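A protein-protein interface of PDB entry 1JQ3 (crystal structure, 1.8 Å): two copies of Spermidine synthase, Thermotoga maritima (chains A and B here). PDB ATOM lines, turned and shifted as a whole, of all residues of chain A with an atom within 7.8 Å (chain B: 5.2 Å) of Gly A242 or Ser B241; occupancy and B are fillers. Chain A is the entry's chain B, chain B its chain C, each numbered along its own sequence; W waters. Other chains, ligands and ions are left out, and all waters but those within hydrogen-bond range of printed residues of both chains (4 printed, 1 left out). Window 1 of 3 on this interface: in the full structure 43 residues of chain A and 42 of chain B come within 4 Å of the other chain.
The side-chain carboxylate (OD2) of Asp A72 lies within hydrogen-bond range of the side-chain hydroxyl (OG1) of Thr A238 (2.7 Å).
The side-chain sulfur of Met A75 sits close to the side-chain hydroxyl of Thr A237 (3.6 Å).
OH of Tyr A273 lies within hydrogen-bond range of N of Phe A235.
O of Gly A242 sits at hydrogen-bond distance from N of Met A236, 3.3 Å away.
N of Tyr B210 lies within hydrogen-bond range of OD2 of Asp B207.
The backbone NH (N) of Met B243 sits close to the side-chain hydroxyl (OG) of Ser B241 (3.2 Å).
Among the printed residues, merely in contact across the chains: Thr A237 with Ser B241, Thr A237 with Phe B209, Phe A235 with Phe B235, Met A243 with Phe B235, Gly A234 with Phe B235, Phe A235 with Met B243, Asp A72 with Phe B209, Leu A233 with Phe B235, Gly A242 with Phe B235, Gly A242 with Ser B241, Phe A235 with Gly B242, Ser A241 with Gly B242 and Thr A238 with Tyr B210.
Asp A207 touches none of the printed residues of chain B.
Phe A209 touches none of the printed residues of chain B.
Printed residues of chain B within 4 Å of Leu A233: Phe B235 (3.8 Å).
Gly A242 touches two residues of chain B.
Of the printed residues of chain A, Phe B235 touches Leu A233 (3.8 Å), Gly A234 (3.5 Å), Phe A235 (3.4 Å), Gly A242 (3.8 Å) and Met A243 (3.5 Å).
Ser B241 touches just these residues of chain A: Thr A237 and Gly A242.
Printed residues of chain A within 4 Å of Gly B242: Phe A235 (3.9 Å) and Ser A241 (3.9 Å).
Of the 10 printed residues of chain B, 6 touch a printed residue of chain A.
Printed residues of chain B that touch a printed residue of chain A: Phe B209, Tyr B210, Phe B235, Ser B241, Gly B242 and Met B243.
Hydrophobic or aromatic side chains of chain B that line the printed part of chain A: Phe B209, Tyr B210, Phe B235 and Met B243.
Phe B235 touches its own counterpart, Phe A235.
Phe A235 touches Gly B242, and with the chains exchanged Gly A242 touches Phe B235.
Phe A235 touches Met B243, and with the chains exchanged Met A243 touches Phe B235.
Ser A241 touches Gly B242, and with the chains exchanged Gly A242 touches Ser B241.
Positions printed for both chains: 23, 207, 209, 210, 235, 239, 240, 241, 242 and 243.
Water W4 bridges the backbone carbonyl oxygen of Thr A237 (2.6 Å) and the side-chain hydroxyl of Tyr B210 (2.6 Å).
Water W3 lies within hydrogen-bond range of O of Gly A242 (2.7 Å), O of Ser B241 (2.8 Å), N of Met A236 (3.2 Å) and N of Met B243 (3.5 Å).
Water W1 lies within hydrogen-bond range of O of Gly B242 (2.7 Å), O of Ser A241 (2.8 Å) and N of Met A243 (3.4 Å).
Water W2 lies within hydrogen-bond range of the backbone carbonyl oxygen of Tyr B239, the backbone carbonyl oxygen of Ser A241 and the backbone NH of Gly B242.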
ATOM      1  N   TYR A  23      -4.461 -21.382  -9.244  1.00  0.00           N
ATOM      2  CA  TYR A  23      -5.518 -22.269  -8.786  1.00  0.00           C
ATOM      3  C   TYR A  23      -4.994 -23.154  -7.664  1.00  0.00           C
ATOM      4  O   TYR A  23      -3.791 -23.208  -7.425  1.00  0.00           O
ATOM      5  CB  TYR A  23      -6.004 -23.149  -9.928  1.00  0.00           C
ATOM      6  CG  TYR A  23      -6.588 -22.351 -11.061  1.00  0.00           C
ATOM      7  CD1 TYR A  23      -7.079 -21.054 -10.853  1.00  0.00           C
ATOM      8  CD2 TYR A  23      -6.690 -22.903 -12.335  1.00  0.00           C
ATOM      9  CE1 TYR A  23      -7.674 -20.333 -11.899  1.00  0.00           C
ATOM     10  CE2 TYR A  23      -7.276 -22.192 -13.379  1.00  0.00           C
ATOM     11  CZ  TYR A  23      -7.772 -20.919 -13.154  1.00  0.00           C
ATOM     12  OH  TYR A  23      -8.433 -20.281 -14.185  1.00  0.00           O
ATOM     13  N   LEU A  30      -4.879 -18.631 -14.215  1.00  0.00           N
ATOM     14  CA  LEU A  30      -5.339 -17.733 -15.261  1.00  0.00           C
ATOM     15  C   LEU A  30      -4.551 -16.430 -15.181  1.00  0.00           C
ATOM     16  O   LEU A  30      -4.193 -15.991 -14.083  1.00  0.00           O
ATOM     17  CB  LEU A  30      -6.818 -17.409 -15.012  1.00  0.00           C
ATOM     18  CG  LEU A  30      -7.581 -16.766 -16.180  1.00  0.00           C
ATOM     19  CD1 LEU A  30      -7.956 -17.856 -17.185  1.00  0.00           C
ATOM     20  CD2 LEU A  30      -8.837 -16.084 -15.657  1.00  0.00           C
ATOM     21  N   ASP A  72     -18.748 -11.157 -17.060  1.00  0.00           N
ATOM     22  CA  ASP A  72     -19.504 -12.382 -16.796  1.00  0.00           C
ATOM     23  C   ASP A  72     -20.052 -12.638 -15.403  1.00  0.00           C
ATOM     24  O   ASP A  72     -20.576 -13.724 -15.164  1.00  0.00           O
ATOM     25  CB  ASP A  72     -18.639 -13.588 -17.196  1.00  0.00           C
ATOM     26  CG  ASP A  72     -17.352 -13.675 -16.383  1.00  0.00           C
ATOM     27  OD1 ASP A  72     -17.211 -12.915 -15.397  1.00  0.00           O
ATOM     28  OD2 ASP A  72     -16.473 -14.511 -16.702  1.00  0.00           O
ATOM     29  N   MET A  75     -23.406 -14.535 -14.802  1.00  0.00           N
ATOM     30  CA  MET A  75     -23.563 -16.003 -14.901  1.00  0.00           C
ATOM     31  C   MET A  75     -23.605 -16.667 -13.520  1.00  0.00           C
ATOM     32  O   MET A  75     -24.357 -17.620 -13.269  1.00  0.00           O
ATOM     33  CB  MET A  75     -22.390 -16.613 -15.673  1.00  0.00           C
ATOM     34  CG  MET A  75     -22.114 -15.987 -17.022  1.00  0.00           C
ATOM     35  SD  MET A  75     -20.865 -16.987 -17.857  1.00  0.00           S
ATOM     36  CE  MET A  75     -20.639 -16.009 -19.367  1.00  0.00           C
ATOM     37  N   ASP A 207     -15.710 -25.627  -7.955  1.00  0.00           N
ATOM     38  CA  ASP A 207     -15.549 -26.434  -9.158  1.00  0.00           C
ATOM     39  C   ASP A 207     -15.162 -27.858  -8.775  1.00  0.00           C
ATOM     40  O   ASP A 207     -14.247 -28.067  -7.964  1.00  0.00           O
ATOM     41  CB  ASP A 207     -14.435 -25.860 -10.051  1.00  0.00           C
ATOM     42  CG  ASP A 207     -13.104 -25.698  -9.309  1.00  0.00           C
ATOM     43  OD1 ASP A 207     -13.014 -24.856  -8.386  1.00  0.00           O
ATOM     44  OD2 ASP A 207     -12.134 -26.395  -9.684  1.00  0.00           O
ATOM     45  N   PRO A 208     -15.851 -28.851  -9.351  1.00  0.00           N
ATOM     46  CA  PRO A 208     -15.551 -30.259  -9.058  1.00  0.00           C
ATOM     47  C   PRO A 208     -14.364 -30.710  -9.923  1.00  0.00           C
ATOM     48  O   PRO A 208     -14.427 -31.738 -10.602  1.00  0.00           O
ATOM     49  CB  PRO A 208     -16.848 -30.965  -9.444  1.00  0.00           C
ATOM     50  CG  PRO A 208     -17.358 -30.132 -10.619  1.00  0.00           C
ATOM     51  CD  PRO A 208     -17.088 -28.709 -10.145  1.00  0.00           C
ATOM     52  N   PHE A 209     -13.302 -29.904  -9.923  1.00  0.00           N
ATOM     53  CA  PHE A 209     -12.105 -30.180 -10.726  1.00  0.00           C
ATOM     54  C   PHE A 209     -10.914 -29.868  -9.816  1.00  0.00           C
ATOM     55  O   PHE A 209     -10.456 -30.751  -9.086  1.00  0.00           O
ATOM     56  CB  PHE A 209     -12.093 -29.297 -12.000  1.00  0.00           C
ATOM     57  CG  PHE A 209     -11.156 -29.792 -13.090  1.00  0.00           C
ATOM     58  CD1 PHE A 209     -11.373 -31.026 -13.710  1.00  0.00           C
ATOM     59  CD2 PHE A 209     -10.050 -29.040 -13.468  1.00  0.00           C
ATOM     60  CE1 PHE A 209     -10.493 -31.508 -14.686  1.00  0.00           C
ATOM     61  CE2 PHE A 209      -9.150 -29.510 -14.457  1.00  0.00           C
ATOM     62  CZ  PHE A 209      -9.377 -30.747 -15.058  1.00  0.00           C
ATOM     63  N   TYR A 210     -10.468 -28.613  -9.781  1.00  0.00           N
ATOM     64  CA  TYR A 210      -9.348 -28.244  -8.904  1.00  0.00           C
ATOM     65  C   TYR A 210      -9.709 -28.291  -7.417  1.00  0.00           C
ATOM     66  O   TYR A 210      -8.850 -28.522  -6.555  1.00  0.00           O
ATOM     67  CB  TYR A 210      -8.857 -26.826  -9.215  1.00  0.00           C
ATOM     68  CG  TYR A 210      -8.357 -26.672 -10.627  1.00  0.00           C
ATOM     69  CD1 TYR A 210      -7.199 -27.328 -11.044  1.00  0.00           C
ATOM     70  CD2 TYR A 210      -9.051 -25.886 -11.557  1.00  0.00           C
ATOM     71  CE1 TYR A 210      -6.740 -27.213 -12.329  1.00  0.00           C
ATOM     72  CE2 TYR A 210      -8.600 -25.769 -12.865  1.00  0.00           C
ATOM     73  CZ  TYR A 210      -7.441 -26.441 -13.242  1.00  0.00           C
ATOM     74  OH  TYR A 210      -7.017 -26.378 -14.546  1.00  0.00           O
ATOM     75  N   LEU A 233     -25.210 -27.154 -11.697  1.00  0.00           N
ATOM     76  CA  LEU A 233     -24.003 -26.624 -12.310  1.00  0.00           C
ATOM     77  C   LEU A 233     -24.270 -25.486 -13.268  1.00  0.00           C
ATOM     78  O   LEU A 233     -25.334 -25.410 -13.893  1.00  0.00           O
ATOM     79  CB  LEU A 233     -23.324 -27.740 -13.120  1.00  0.00           C
ATOM     80  CG  LEU A 233     -23.098 -29.071 -12.406  1.00  0.00           C
ATOM     81  CD1 LEU A 233     -22.695 -30.167 -13.430  1.00  0.00           C
ATOM     82  CD2 LEU A 233     -22.027 -28.901 -11.347  1.00  0.00           C
ATOM     83  N   GLY A 234     -23.257 -24.645 -13.432  1.00  0.00           N
ATOM     84  CA  GLY A 234     -23.384 -23.551 -14.370  1.00  0.00           C
ATOM     85  C   GLY A 234     -22.025 -23.154 -14.892  1.00  0.00           C
ATOM     86  O   GLY A 234     -20.996 -23.434 -14.269  1.00  0.00           O
ATOM     87  N   PHE A 235     -22.020 -22.526 -16.060  1.00  0.00           N
ATOM     88  CA  PHE A 235     -20.778 -22.032 -16.634  1.00  0.00           C
ATOM     89  C   PHE A 235     -20.403 -20.751 -15.877  1.00  0.00           C
ATOM     90  O   PHE A 235     -21.268 -20.033 -15.383  1.00  0.00           O
ATOM     91  CB  PHE A 235     -20.982 -21.734 -18.117  1.00  0.00           C
ATOM     92  CG  PHE A 235     -21.294 -22.952 -18.929  1.00  0.00           C
ATOM     93  CD1 PHE A 235     -20.288 -23.858 -19.245  1.00  0.00           C
ATOM     94  CD2 PHE A 235     -22.596 -23.216 -19.353  1.00  0.00           C
ATOM     95  CE1 PHE A 235     -20.581 -25.025 -19.980  1.00  0.00           C
ATOM     96  CE2 PHE A 235     -22.893 -24.376 -20.082  1.00  0.00           C
ATOM     97  CZ  PHE A 235     -21.877 -25.277 -20.391  1.00  0.00           C
ATOM     98  N   MET A 236     -19.110 -20.516 -15.701  1.00  0.00           N
ATOM     99  CA  MET A 236     -18.629 -19.314 -15.012  1.00  0.00           C
ATOM    100  C   MET A 236     -17.291 -19.147 -15.708  1.00  0.00           C
ATOM    101  O   MET A 236     -16.275 -19.714 -15.314  1.00  0.00           O
ATOM    102  CB  MET A 236     -18.454 -19.576 -13.526  1.00  0.00           C
ATOM    103  CG  MET A 236     -18.640 -18.355 -12.682  1.00  0.00           C
ATOM    104  SD  MET A 236     -17.514 -17.022 -13.158  1.00  0.00           S
ATOM    105  CE  MET A 236     -18.730 -15.997 -13.969  1.00  0.00           C
ATOM    106  N   THR A 237     -17.342 -18.358 -16.768  1.00  0.00           N
ATOM    107  CA  THR A 237     -16.240 -18.164 -17.676  1.00  0.00           C
ATOM    108  C   THR A 237     -14.908 -17.652 -17.178  1.00  0.00           C
ATOM    109  O   THR A 237     -13.933 -17.706 -17.929  1.00  0.00           O
ATOM    110  CB  THR A 237     -16.710 -17.389 -18.919  1.00  0.00           C
ATOM    111  OG1 THR A 237     -17.421 -16.229 -18.506  1.00  0.00           O
ATOM    112  CG2 THR A 237     -17.650 -18.255 -19.772  1.00  0.00           C
ATOM    113  N   THR A 238     -14.843 -17.175 -15.939  1.00  0.00           N
ATOM    114  CA  THR A 238     -13.560 -16.719 -15.408  1.00  0.00           C
ATOM    115  C   THR A 238     -13.191 -17.318 -14.044  1.00  0.00           C
ATOM    116  O   THR A 238     -12.241 -16.864 -13.393  1.00  0.00           O
ATOM    117  CB  THR A 238     -13.418 -15.173 -15.388  1.00  0.00           C
ATOM    118  OG1 THR A 238     -14.581 -14.577 -14.806  1.00  0.00           O
ATOM    119  CG2 THR A 238     -13.213 -14.626 -16.804  1.00  0.00           C
ATOM    120  N   TYR A 239     -13.967 -18.302 -13.591  1.00  0.00           N
ATOM    121  CA  TYR A 239     -13.666 -18.985 -12.330  1.00  0.00           C
ATOM    122  C   TYR A 239     -12.847 -20.221 -12.713  1.00  0.00           C
ATOM    123  O   TYR A 239     -12.972 -20.743 -13.824  1.00  0.00           O
ATOM    124  CB  TYR A 239     -14.942 -19.416 -11.599  1.00  0.00           C
ATOM    125  CG  TYR A 239     -15.534 -18.351 -10.705  1.00  0.00           C
ATOM    126  CD1 TYR A 239     -14.923 -17.099 -10.563  1.00  0.00           C
ATOM    127  CD2 TYR A 239     -16.702 -18.595  -9.997  1.00  0.00           C
ATOM    128  CE1 TYR A 239     -15.470 -16.115  -9.726  1.00  0.00           C
ATOM    129  CE2 TYR A 239     -17.256 -17.618  -9.167  1.00  0.00           C
ATOM    130  CZ  TYR A 239     -16.630 -16.386  -9.043  1.00  0.00           C
ATOM    131  OH  TYR A 239     -17.206 -15.428  -8.250  1.00  0.00           O
ATOM    132  N   PRO A 240     -12.071 -20.757 -11.767  1.00  0.00           N
ATOM    133  CA  PRO A 240     -11.241 -21.932 -12.031  1.00  0.00           C
ATOM    134  C   PRO A 240     -11.997 -23.108 -12.672  1.00  0.00           C
ATOM    135  O   PRO A 240     -12.940 -23.652 -12.100  1.00  0.00           O
ATOM    136  CB  PRO A 240     -10.683 -22.283 -10.646  1.00  0.00           C
ATOM    137  CG  PRO A 240     -10.707 -20.937  -9.888  1.00  0.00           C
ATOM    138  CD  PRO A 240     -12.015 -20.351 -10.348  1.00  0.00           C
ATOM    139  N   SER A 241     -11.518 -23.507 -13.848  1.00  0.00           N
ATOM    140  CA  SER A 241     -12.066 -24.615 -14.642  1.00  0.00           C
ATOM    141  C   SER A 241     -13.281 -24.246 -15.479  1.00  0.00           C
ATOM    142  O   SER A 241     -13.590 -24.948 -16.430  1.00  0.00           O
ATOM    143  CB  SER A 241     -12.405 -25.842 -13.774  1.00  0.00           C
ATOM    144  OG  SER A 241     -13.740 -25.802 -13.289  1.00  0.00           O
ATOM    145  N   GLY A 242     -13.972 -23.164 -15.125  1.00  0.00           N
ATOM    146  CA  GLY A 242     -15.167 -22.771 -15.874  1.00  0.00           C
ATOM    147  C   GLY A 242     -16.395 -23.611 -15.540  1.00  0.00           C
ATOM    148  O   GLY A 242     -17.493 -23.355 -16.042  1.00  0.00           O
ATOM    149  N   MET A 243     -16.219 -24.634 -14.705  1.00  0.00           N
ATOM    150  CA  MET A 243     -17.345 -25.491 -14.333  1.00  0.00           C
ATOM    151  C   MET A 243     -17.644 -25.238 -12.862  1.00  0.00           C
ATOM    152  O   MET A 243     -16.949 -25.742 -11.981  1.00  0.00           O
ATOM    153  CB  MET A 243     -16.986 -26.963 -14.586  1.00  0.00           C
ATOM    154  CG  MET A 243     -18.123 -27.928 -14.236  1.00  0.00           C
ATOM    155  SD  MET A 243     -17.641 -29.644 -14.538  1.00  0.00           S
ATOM    156  CE  MET A 243     -19.121 -30.478 -14.179  1.00  0.00           C
ATOM    157  N   TRP A 244     -18.695 -24.470 -12.593  1.00  0.00           N
ATOM    158  CA  TRP A 244     -19.028 -24.134 -11.217  1.00  0.00           C
ATOM    159  C   TRP A 244     -20.221 -24.901 -10.694  1.00  0.00           C
ATOM    160  O   TRP A 244     -21.151 -25.205 -11.450  1.00  0.00           O
ATOM    161  CB  TRP A 244     -19.279 -22.632 -11.092  1.00  0.00           C
ATOM    162  CG  TRP A 244     -18.766 -22.109  -9.817  1.00  0.00           C
ATOM    163  CD1 TRP A 244     -19.493 -21.608  -8.770  1.00  0.00           C
ATOM    164  CD2 TRP A 244     -17.400 -22.097  -9.404  1.00  0.00           C
ATOM    165  NE1 TRP A 244     -18.652 -21.294  -7.723  1.00  0.00           N
ATOM    166  CE2 TRP A 244     -17.362 -21.580  -8.089  1.00  0.00           C
ATOM    167  CE3 TRP A 244     -16.202 -22.483 -10.019  1.00  0.00           C
ATOM    168  CZ2 TRP A 244     -16.164 -21.431  -7.372  1.00  0.00           C
ATOM    169  CZ3 TRP A 244     -15.004 -22.338  -9.312  1.00  0.00           C
ATOM    170  CH2 TRP A 244     -14.997 -21.815  -7.996  1.00  0.00           C
ATOM    171  N   SER A 245     -20.156 -25.284  -9.420  1.00  0.00           N
ATOM    172  CA  SER A 245     -21.269 -25.992  -8.796  1.00  0.00           C
ATOM    173  C   SER A 245     -21.914 -25.129  -7.712  1.00  0.00           C
ATOM    174  O   SER A 245     -21.272 -24.282  -7.069  1.00  0.00           O
ATOM    175  CB  SER A 245     -20.822 -27.330  -8.166  1.00  0.00           C
ATOM    176  OG  SER A 245     -20.166 -27.109  -6.916  1.00  0.00           O
ATOM    177  N   TYR A 273     -28.654 -14.882 -18.170  1.00  0.00           N
ATOM    178  CA  TYR A 273     -28.223 -16.286 -18.213  1.00  0.00           C
ATOM    179  C   TYR A 273     -29.387 -17.242 -17.916  1.00  0.00           C
ATOM    180  O   TYR A 273     -29.797 -18.042 -18.761  1.00  0.00           O
ATOM    181  CB  TYR A 273     -27.075 -16.501 -17.203  1.00  0.00           C
ATOM    182  CG  TYR A 273     -26.463 -17.900 -17.194  1.00  0.00           C
ATOM    183  CD1 TYR A 273     -27.121 -18.972 -16.580  1.00  0.00           C
ATOM    184  CD2 TYR A 273     -25.223 -18.147 -17.797  1.00  0.00           C
ATOM    185  CE1 TYR A 273     -26.555 -20.258 -16.565  1.00  0.00           C
ATOM    186  CE2 TYR A 273     -24.656 -19.424 -17.790  1.00  0.00           C
ATOM    187  CZ  TYR A 273     -25.336 -20.477 -17.172  1.00  0.00           C
ATOM    188  OH  TYR A 273     -24.832 -21.757 -17.213  1.00  0.00           O
ATOM    189  N   TYR B  23      -5.587 -16.451 -25.057  1.00  0.00           N
ATOM    190  CA  TYR B  23      -6.916 -16.587 -25.620  1.00  0.00           C
ATOM    191  C   TYR B  23      -7.091 -15.516 -26.692  1.00  0.00           C
ATOM    192  O   TYR B  23      -6.292 -14.572 -26.775  1.00  0.00           O
ATOM    193  CB  TYR B  23      -7.968 -16.379 -24.529  1.00  0.00           C
ATOM    194  CG  TYR B  23      -7.902 -17.395 -23.404  1.00  0.00           C
ATOM    195  CD1 TYR B  23      -7.290 -18.639 -23.593  1.00  0.00           C
ATOM    196  CD2 TYR B  23      -8.514 -17.135 -22.173  1.00  0.00           C
ATOM    197  CE1 TYR B  23      -7.302 -19.610 -22.583  1.00  0.00           C
ATOM    198  CE2 TYR B  23      -8.525 -18.088 -21.167  1.00  0.00           C
ATOM    199  CZ  TYR B  23      -7.924 -19.323 -21.387  1.00  0.00           C
ATOM    200  OH  TYR B  23      -7.993 -20.281 -20.412  1.00  0.00           O
ATOM    201  N   ASP B 207     -15.960 -21.541 -28.062  1.00  0.00           N
ATOM    202  CA  ASP B 207     -16.533 -20.973 -26.852  1.00  0.00           C
ATOM    203  C   ASP B 207     -17.232 -19.681 -27.230  1.00  0.00           C
ATOM    204  O   ASP B 207     -16.648 -18.820 -27.906  1.00  0.00           O
ATOM    205  CB  ASP B 207     -15.420 -20.640 -25.837  1.00  0.00           C
ATOM    206  CG  ASP B 207     -14.373 -19.681 -26.413  1.00  0.00           C
ATOM    207  OD1 ASP B 207     -13.671 -20.072 -27.356  1.00  0.00           O
ATOM    208  OD2 ASP B 207     -14.271 -18.537 -25.930  1.00  0.00           O
ATOM    209  N   PHE B 209     -17.691 -17.003 -25.865  1.00  0.00           N
ATOM    210  CA  PHE B 209     -17.236 -15.981 -24.923  1.00  0.00           C
ATOM    211  C   PHE B 209     -16.107 -15.228 -25.625  1.00  0.00           C
ATOM    212  O   PHE B 209     -16.362 -14.224 -26.276  1.00  0.00           O
ATOM    213  CB  PHE B 209     -16.762 -16.619 -23.609  1.00  0.00           C
ATOM    214  CG  PHE B 209     -16.557 -15.617 -22.488  1.00  0.00           C
ATOM    215  CD1 PHE B 209     -17.632 -14.879 -21.994  1.00  0.00           C
ATOM    216  CD2 PHE B 209     -15.299 -15.422 -21.935  1.00  0.00           C
ATOM    217  CE1 PHE B 209     -17.451 -13.958 -20.961  1.00  0.00           C
ATOM    218  CE2 PHE B 209     -15.097 -14.500 -20.896  1.00  0.00           C
ATOM    219  CZ  PHE B 209     -16.167 -13.770 -20.412  1.00  0.00           C
ATOM    220  N   TYR B 210     -14.888 -15.760 -25.590  1.00  0.00           N
ATOM    221  CA  TYR B 210     -13.763 -15.106 -26.272  1.00  0.00           C
ATOM    222  C   TYR B 210     -13.890 -15.226 -27.801  1.00  0.00           C
ATOM    223  O   TYR B 210     -13.353 -14.394 -28.530  1.00  0.00           O
ATOM    224  CB  TYR B 210     -12.427 -15.728 -25.841  1.00  0.00           C
ATOM    225  CG  TYR B 210     -12.157 -15.570 -24.373  1.00  0.00           C
ATOM    226  CD1 TYR B 210     -11.929 -14.298 -23.824  1.00  0.00           C
ATOM    227  CD2 TYR B 210     -12.143 -16.681 -23.512  1.00  0.00           C
ATOM    228  CE1 TYR B 210     -11.699 -14.139 -22.468  1.00  0.00           C
ATOM    229  CE2 TYR B 210     -11.909 -16.527 -22.150  1.00  0.00           C
ATOM    230  CZ  TYR B 210     -11.690 -15.251 -21.638  1.00  0.00           C
ATOM    231  OH  TYR B 210     -11.489 -15.070 -20.293  1.00  0.00           O
ATOM    232  N   PHE B 235     -19.129 -28.573 -20.517  1.00  0.00           N
ATOM    233  CA  PHE B 235     -18.000 -28.063 -19.761  1.00  0.00           C
ATOM    234  C   PHE B 235     -16.735 -28.654 -20.402  1.00  0.00           C
ATOM    235  O   PHE B 235     -16.771 -29.725 -20.961  1.00  0.00           O
ATOM    236  CB  PHE B 235     -18.109 -28.502 -18.309  1.00  0.00           C
ATOM    237  CG  PHE B 235     -19.276 -27.890 -17.586  1.00  0.00           C
ATOM    238  CD1 PHE B 235     -19.248 -26.543 -17.216  1.00  0.00           C
ATOM    239  CD2 PHE B 235     -20.410 -28.649 -17.297  1.00  0.00           C
ATOM    240  CE1 PHE B 235     -20.338 -25.963 -16.569  1.00  0.00           C
ATOM    241  CE2 PHE B 235     -21.516 -28.078 -16.648  1.00  0.00           C
ATOM    242  CZ  PHE B 235     -21.475 -26.733 -16.285  1.00  0.00           C
ATOM    243  N   TYR B 239     -10.238 -25.641 -21.680  1.00  0.00           N
ATOM    244  CA  TYR B 239     -10.395 -24.871 -22.931  1.00  0.00           C
ATOM    245  C   TYR B 239     -10.743 -23.432 -22.546  1.00  0.00           C
ATOM    246  O   TYR B 239     -11.345 -23.205 -21.498  1.00  0.00           O
ATOM    247  CB  TYR B 239     -11.498 -25.437 -23.820  1.00  0.00           C
ATOM    248  CG  TYR B 239     -11.054 -26.573 -24.724  1.00  0.00           C
ATOM    249  CD1 TYR B 239      -9.723 -27.009 -24.743  1.00  0.00           C
ATOM    250  CD2 TYR B 239     -11.971 -27.213 -25.554  1.00  0.00           C
ATOM    251  CE1 TYR B 239      -9.321 -28.065 -25.576  1.00  0.00           C
ATOM    252  CE2 TYR B 239     -11.585 -28.265 -26.382  1.00  0.00           C
ATOM    253  CZ  TYR B 239     -10.257 -28.686 -26.386  1.00  0.00           C
ATOM    254  OH  TYR B 239      -9.871 -29.740 -27.204  1.00  0.00           O
ATOM    255  N   PRO B 240     -10.495 -22.461 -23.452  1.00  0.00           N
ATOM    256  CA  PRO B 240     -10.788 -21.047 -23.157  1.00  0.00           C
ATOM    257  C   PRO B 240     -12.217 -20.804 -22.687  1.00  0.00           C
ATOM    258  O   PRO B 240     -13.166 -21.114 -23.416  1.00  0.00           O
ATOM    259  CB  PRO B 240     -10.498 -20.358 -24.496  1.00  0.00           C
ATOM    260  CG  PRO B 240      -9.388 -21.218 -25.077  1.00  0.00           C
ATOM    261  CD  PRO B 240      -9.902 -22.606 -24.801  1.00  0.00           C
ATOM    262  N   SER B 241     -12.337 -20.237 -21.479  1.00  0.00           N
ATOM    263  CA  SER B 241     -13.610 -19.914 -20.799  1.00  0.00           C
ATOM    264  C   SER B 241     -14.279 -21.096 -20.107  1.00  0.00           C
ATOM    265  O   SER B 241     -15.139 -20.897 -19.246  1.00  0.00           O
ATOM    266  CB  SER B 241     -14.634 -19.241 -21.728  1.00  0.00           C
ATOM    267  OG  SER B 241     -15.413 -20.182 -22.448  1.00  0.00           O
ATOM    268  N   GLY B 242     -13.942 -22.316 -20.521  1.00  0.00           N
ATOM    269  CA  GLY B 242     -14.546 -23.484 -19.907  1.00  0.00           C
ATOM    270  C   GLY B 242     -15.961 -23.757 -20.389  1.00  0.00           C
ATOM    271  O   GLY B 242     -16.589 -24.714 -19.949  1.00  0.00           O
ATOM    272  N   MET B 243     -16.480 -22.914 -21.276  1.00  0.00           N
ATOM    273  CA  MET B 243     -17.832 -23.121 -21.805  1.00  0.00           C
ATOM    274  C   MET B 243     -17.693 -23.451 -23.289  1.00  0.00           C
ATOM    275  O   MET B 243     -17.425 -22.559 -24.098  1.00  0.00           O
ATOM    276  CB  MET B 243     -18.669 -21.853 -21.621  1.00  0.00           C
ATOM    277  CG  MET B 243     -20.070 -21.985 -22.193  1.00  0.00           C
ATOM    278  SD  MET B 243     -20.978 -20.451 -21.918  1.00  0.00           S
ATOM    279  CE  MET B 243     -22.620 -20.988 -22.155  1.00  0.00           C
HETATM  280  O   HOH W   1     -15.744 -26.089 -17.753  1.00  0.00           O
HETATM  281  O   HOH W   2     -11.529 -24.030 -18.883  1.00  0.00           O
HETATM  282  O   HOH W   3     -17.571 -21.762 -18.170  1.00  0.00           O
HETATM  283  O   HOH W   4     -11.533 -17.248 -18.789  1.00  0.00           O
